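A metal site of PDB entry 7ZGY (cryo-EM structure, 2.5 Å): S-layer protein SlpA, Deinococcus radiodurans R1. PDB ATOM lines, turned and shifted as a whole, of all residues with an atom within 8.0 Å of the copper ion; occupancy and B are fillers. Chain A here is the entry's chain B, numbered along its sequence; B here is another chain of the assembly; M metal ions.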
ATOM      1  N   ARG A 519      33.908 -17.583  12.701  1.00  0.00           N
ATOM      2  CA  ARG A 519      33.464 -16.192  12.744  1.00  0.00           C
ATOM      3  C   ARG A 519      32.625 -15.794  11.541  1.00  0.00           C
ATOM      4  O   ARG A 519      31.653 -15.052  11.703  1.00  0.00           O
ATOM      5  CB  ARG A 519      34.673 -15.259  12.860  1.00  0.00           C
ATOM      6  CG  ARG A 519      34.310 -13.850  13.286  1.00  0.00           C
ATOM      7  CD  ARG A 519      35.478 -13.168  13.964  1.00  0.00           C
ATOM      8  NE  ARG A 519      35.052 -12.063  14.810  1.00  0.00           N
ATOM      9  CZ  ARG A 519      34.575 -12.200  16.035  1.00  0.00           C
ATOM     10  NH1 ARG A 519      34.411 -13.398  16.581  1.00  0.00           N
ATOM     11  NH2 ARG A 519      34.242 -11.126  16.733  1.00  0.00           N
ATOM     12  N   GLY A 520      32.968 -16.261  10.352  1.00  0.00           N
ATOM     13  CA  GLY A 520      32.223 -15.845   9.172  1.00  0.00           C
ATOM     14  C   GLY A 520      32.761 -16.509   7.929  1.00  0.00           C
ATOM     15  O   GLY A 520      33.471 -17.516   7.989  1.00  0.00           O
ATOM     16  N   ASP A 521      32.404 -15.916   6.797  1.00  0.00           N
ATOM     17  CA  ASP A 521      32.724 -16.476   5.486  1.00  0.00           C
ATOM     18  C   ASP A 521      33.912 -15.745   4.875  1.00  0.00           C
ATOM     19  O   ASP A 521      33.945 -14.514   4.872  1.00  0.00           O
ATOM     20  CB  ASP A 521      31.529 -16.391   4.547  1.00  0.00           C
ATOM     21  CG  ASP A 521      30.298 -17.066   5.112  1.00  0.00           C
ATOM     22  OD1 ASP A 521      30.418 -17.756   6.141  1.00  0.00           O
ATOM     23  OD2 ASP A 521      29.209 -16.920   4.519  1.00  0.00           O
ATOM     24  N   GLY A 547      37.723 -12.311   6.383  1.00  0.00           N
ATOM     25  CA  GLY A 547      36.360 -12.790   6.291  1.00  0.00           C
ATOM     26  C   GLY A 547      35.339 -11.727   6.621  1.00  0.00           C
ATOM     27  O   GLY A 547      35.674 -10.629   7.087  1.00  0.00           O
ATOM     28  N   SER A 548      34.086 -12.069   6.365  1.00  0.00           N
ATOM     29  CA  SER A 548      32.928 -11.269   6.711  1.00  0.00           C
ATOM     30  C   SER A 548      32.152 -11.995   7.804  1.00  0.00           C
ATOM     31  O   SER A 548      31.804 -13.162   7.637  1.00  0.00           O
ATOM     32  CB  SER A 548      32.026 -11.035   5.487  1.00  0.00           C
ATOM     33  OG  SER A 548      30.858 -10.333   5.836  1.00  0.00           O
ATOM     34  N   ARG A 549      31.891 -11.294   8.904  1.00  0.00           N
ATOM     35  CA  ARG A 549      31.247 -11.929  10.059  1.00  0.00           C
ATOM     36  C   ARG A 549      29.878 -12.476   9.678  1.00  0.00           C
ATOM     37  O   ARG A 549      29.064 -11.779   9.070  1.00  0.00           O
ATOM     38  CB  ARG A 549      31.106 -10.933  11.199  1.00  0.00           C
ATOM     39  CG  ARG A 549      32.110 -11.118  12.308  1.00  0.00           C
ATOM     40  CD  ARG A 549      31.771 -10.229  13.497  1.00  0.00           C
ATOM     41  NE  ARG A 549      30.723 -10.791  14.327  1.00  0.00           N
ATOM     42  CZ  ARG A 549      30.334 -10.279  15.486  1.00  0.00           C
ATOM     43  NH1 ARG A 549      30.892  -9.175  15.975  1.00  0.00           N
ATOM     44  NH2 ARG A 549      29.363 -10.875  16.173  1.00  0.00           N
ATOM     45  N   SER A 550      29.623 -13.730  10.048  1.00  0.00           N
ATOM     46  CA  SER A 550      28.340 -14.378   9.829  1.00  0.00           C
ATOM     47  C   SER A 550      27.926 -14.371   8.364  1.00  0.00           C
ATOM     48  O   SER A 550      26.755 -14.580   8.049  1.00  0.00           O
ATOM     49  CB  SER A 550      27.250 -13.748  10.685  1.00  0.00           C
ATOM     50  OG  SER A 550      27.600 -13.771  12.060  1.00  0.00           O
ATOM     51  N   GLY A 551      28.865 -14.147   7.455  1.00  0.00           N
ATOM     52  CA  GLY A 551      28.495 -14.003   6.061  1.00  0.00           C
ATOM     53  C   GLY A 551      27.554 -12.836   5.883  1.00  0.00           C
ATOM     54  O   GLY A 551      27.712 -11.775   6.504  1.00  0.00           O
ATOM     55  N   LEU A 552      26.555 -13.015   5.029  1.00  0.00           N
ATOM     56  CA  LEU A 552      25.532 -11.998   4.824  1.00  0.00           C
ATOM     57  C   LEU A 552      24.357 -12.275   5.750  1.00  0.00           C
ATOM     58  O   LEU A 552      23.823 -13.378   5.782  1.00  0.00           O
ATOM     59  CB  LEU A 552      25.071 -11.965   3.366  1.00  0.00           C
ATOM     60  CG  LEU A 552      24.393 -13.193   2.784  1.00  0.00           C
ATOM     61  CD1 LEU A 552      22.897 -13.146   3.022  1.00  0.00           C
ATOM     62  CD2 LEU A 552      24.687 -13.287   1.298  1.00  0.00           C
ATOM     63  N   ASP A 553      23.969 -11.257   6.519  1.00  0.00           N
ATOM     64  CA  ASP A 553      22.900 -11.390   7.499  1.00  0.00           C
ATOM     65  C   ASP A 553      22.146 -10.081   7.594  1.00  0.00           C
ATOM     66  O   ASP A 553      22.700  -9.006   7.359  1.00  0.00           O
ATOM     67  CB  ASP A 553      23.447 -11.817   8.860  1.00  0.00           C
ATOM     68  CG  ASP A 553      24.509 -10.866   9.377  1.00  0.00           C
ATOM     69  OD1 ASP A 553      24.729  -9.823   8.748  1.00  0.00           O
ATOM     70  OD2 ASP A 553      25.116 -11.173  10.425  1.00  0.00           O
ATOM     71  N   GLY A 554      20.858 -10.178   7.931  1.00  0.00           N
ATOM     72  CA  GLY A 554      20.010  -9.003   7.945  1.00  0.00           C
ATOM     73  C   GLY A 554      20.441  -7.994   8.986  1.00  0.00           C
ATOM     74  O   GLY A 554      21.099  -8.297   9.974  1.00  0.00           O
ATOM     75  N   GLU A 557      21.623  -7.406  13.111  1.00  0.00           N
ATOM     76  CA  GLU A 557      22.493  -8.501  13.512  1.00  0.00           C
ATOM     77  C   GLU A 557      23.909  -7.975  13.701  1.00  0.00           C
ATOM     78  O   GLU A 557      24.360  -7.070  12.992  1.00  0.00           O
ATOM     79  CB  GLU A 557      22.493  -9.614  12.465  1.00  0.00           C
ATOM     80  CG  GLU A 557      21.160 -10.302  12.294  1.00  0.00           C
ATOM     81  CD  GLU A 557      21.266 -11.642  11.590  1.00  0.00           C
ATOM     82  OE1 GLU A 557      22.170 -12.419  11.937  1.00  0.00           O
ATOM     83  OE2 GLU A 557      20.453 -11.911  10.680  1.00  0.00           O
ATOM     84  N   ALA A 558      24.607  -8.542  14.686  1.00  0.00           N
ATOM     85  CA  ALA A 558      25.933  -8.051  15.041  1.00  0.00           C
ATOM     86  C   ALA A 558      26.929  -8.183  13.903  1.00  0.00           C
ATOM     87  O   ALA A 558      27.950  -7.489  13.913  1.00  0.00           O
ATOM     88  CB  ALA A 558      26.448  -8.780  16.278  1.00  0.00           C
ATOM     89  N   GLY A 559      26.673  -9.054  12.941  1.00  0.00           N
ATOM     90  CA  GLY A 559      27.624  -9.309  11.880  1.00  0.00           C
ATOM     91  C   GLY A 559      27.279  -8.666  10.548  1.00  0.00           C
ATOM     92  O   GLY A 559      27.711  -9.146   9.498  1.00  0.00           O
ATOM     93  N   TYR A 560      26.507  -7.587  10.575  1.00  0.00           N
ATOM     94  CA  TYR A 560      26.130  -6.882   9.354  1.00  0.00           C
ATOM     95  C   TYR A 560      27.181  -5.846   9.014  1.00  0.00           C
ATOM     96  O   TYR A 560      27.460  -4.952   9.823  1.00  0.00           O
ATOM     97  CB  TYR A 560      24.755  -6.216   9.501  1.00  0.00           C
ATOM     98  CG  TYR A 560      24.299  -5.537   8.241  1.00  0.00           C
ATOM     99  CD1 TYR A 560      23.670  -6.254   7.234  1.00  0.00           C
ATOM    100  CD2 TYR A 560      24.522  -4.188   8.032  1.00  0.00           C
ATOM    101  CE1 TYR A 560      23.261  -5.651   6.071  1.00  0.00           C
ATOM    102  CE2 TYR A 560      24.116  -3.568   6.869  1.00  0.00           C
ATOM    103  CZ  TYR A 560      23.487  -4.303   5.899  1.00  0.00           C
ATOM    104  OH  TYR A 560      23.073  -3.687   4.731  1.00  0.00           O
ATOM    105  N   GLY A 561      27.766  -5.963   7.835  1.00  0.00           N
ATOM    106  CA  GLY A 561      28.775  -5.023   7.404  1.00  0.00           C
ATOM    107  C   GLY A 561      30.013  -5.003   8.266  1.00  0.00           C
ATOM    108  O   GLY A 561      30.694  -3.975   8.342  1.00  0.00           O
ATOM    109  N   VAL A 562      30.320  -6.110   8.931  1.00  0.00           N
ATOM    110  CA  VAL A 562      31.513  -6.234   9.767  1.00  0.00           C
ATOM    111  C   VAL A 562      32.446  -7.240   9.118  1.00  0.00           C
ATOM    112  O   VAL A 562      32.030  -8.367   8.798  1.00  0.00           O
ATOM    113  CB  VAL A 562      31.171  -6.641  11.209  1.00  0.00           C
ATOM    114  CG1 VAL A 562      30.447  -5.515  11.921  1.00  0.00           C
ATOM    115  CG2 VAL A 562      30.339  -7.890  11.213  1.00  0.00           C
ATOM    116  N   TYR A 563      33.697  -6.846   8.933  1.00  0.00           N
ATOM    117  CA  TYR A 563      34.712  -7.691   8.319  1.00  0.00           C
ATOM    118  C   TYR A 563      35.915  -7.754   9.226  1.00  0.00           C
ATOM    119  O   TYR A 563      36.264  -6.769   9.891  1.00  0.00           O
ATOM    120  CB  TYR A 563      35.099  -7.164   6.923  1.00  0.00           C
ATOM    121  CG  TYR A 563      33.929  -7.106   5.971  1.00  0.00           C
ATOM    122  CD1 TYR A 563      33.035  -6.058   6.008  1.00  0.00           C
ATOM    123  CD2 TYR A 563      33.714  -8.121   5.055  1.00  0.00           C
ATOM    124  CE1 TYR A 563      31.968  -6.009   5.150  1.00  0.00           C
ATOM    125  CE2 TYR A 563      32.638  -8.082   4.201  1.00  0.00           C
ATOM    126  CZ  TYR A 563      31.773  -7.016   4.257  1.00  0.00           C
ATOM    127  OH  TYR A 563      30.693  -6.964   3.398  1.00  0.00           O
ATOM    128  N   TYR B 379      24.730  -2.663  -2.049  1.00  0.00           N
ATOM    129  CA  TYR B 379      25.653  -3.402  -1.206  1.00  0.00           C
ATOM    130  C   TYR B 379      25.488  -4.886  -1.442  1.00  0.00           C
ATOM    131  O   TYR B 379      24.366  -5.383  -1.575  1.00  0.00           O
ATOM    132  CB  TYR B 379      25.430  -3.080   0.272  1.00  0.00           C
ATOM    133  CG  TYR B 379      26.479  -3.667   1.193  1.00  0.00           C
ATOM    134  CD1 TYR B 379      27.827  -3.644   0.855  1.00  0.00           C
ATOM    135  CD2 TYR B 379      26.124  -4.213   2.420  1.00  0.00           C
ATOM    136  CE1 TYR B 379      28.781  -4.166   1.698  1.00  0.00           C
ATOM    137  CE2 TYR B 379      27.077  -4.740   3.271  1.00  0.00           C
ATOM    138  CZ  TYR B 379      28.400  -4.713   2.905  1.00  0.00           C
ATOM    139  OH  TYR B 379      29.356  -5.229   3.740  1.00  0.00           O
ATOM    140  N   GLU B 381      26.805  -7.814   0.794  1.00  0.00           N
ATOM    141  CA  GLU B 381      27.532  -8.198   1.992  1.00  0.00           C
ATOM    142  C   GLU B 381      28.370  -9.442   1.714  1.00  0.00           C
ATOM    143  O   GLU B 381      27.872 -10.426   1.150  1.00  0.00           O
ATOM    144  CB  GLU B 381      26.565  -8.453   3.149  1.00  0.00           C
ATOM    145  CG  GLU B 381      27.211  -8.282   4.511  1.00  0.00           C
ATOM    146  CD  GLU B 381      26.334  -8.792   5.621  1.00  0.00           C
ATOM    147  OE1 GLU B 381      25.098  -8.775   5.463  1.00  0.00           O
ATOM    148  OE2 GLU B 381      26.876  -9.227   6.661  1.00  0.00           O
ATOM    149  N   GLY B 382      29.633  -9.392   2.114  1.00  0.00           N
ATOM    150  CA  GLY B 382      30.540 -10.472   1.808  1.00  0.00           C
ATOM    151  C   GLY B 382      30.085 -11.811   2.330  1.00  0.00           C
ATOM    152  O   GLY B 382      29.757 -11.950   3.516  1.00  0.00           O
ATOM    153  N   SER B 383      30.035 -12.808   1.455  1.00  0.00           N
ATOM    154  CA  SER B 383      29.685 -14.157   1.871  1.00  0.00           C
ATOM    155  C   SER B 383      30.283 -15.155   0.894  1.00  0.00           C
ATOM    156  O   SER B 383      30.601 -14.809  -0.260  1.00  0.00           O
ATOM    157  CB  SER B 383      28.170 -14.350   1.970  1.00  0.00           C
ATOM    158  OG  SER B 383      27.597 -14.460   0.683  1.00  0.00           O
HETATM  159 CU    CU M   1      27.999 -10.176   7.931  1.00  0.00          CU
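OG of Ser 548 sits at hydrogen-bond distance from O of Gly 382 of chain B, at 3.0 Å. The side-chain carboxylate (OE1) of Glu 381 of chain B is in hydrogen-bond range of the backbone NH (N) of Asp 553. O of Asp 521 lies within hydrogen-bond range of N of Ser 548 (2.9 Å). O of Val 562 is in hydrogen-bond range of N of Arg 549 (2.9 Å). The side-chain carboxylate (OD1) of Asp 553 sits close to the backbone NH (N) of Tyr 560.
Residues that only touch the copper ion: Ser 548, Asp 553 and Tyr 560. Seven residues have an atom within 4 Å of the copper ion: Ser 548, Arg 549, Gly 551, Asp 553, Gly 559, Tyr 560 and Glu 381 of chain B. The nearest printed residue that does not touch the copper ion is Ser 550 (4.2 Å).
The copper ion is bound by O of Gly 559, OE2 of Glu 381 of chain B, O of Gly 551 and O of Arg 549.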
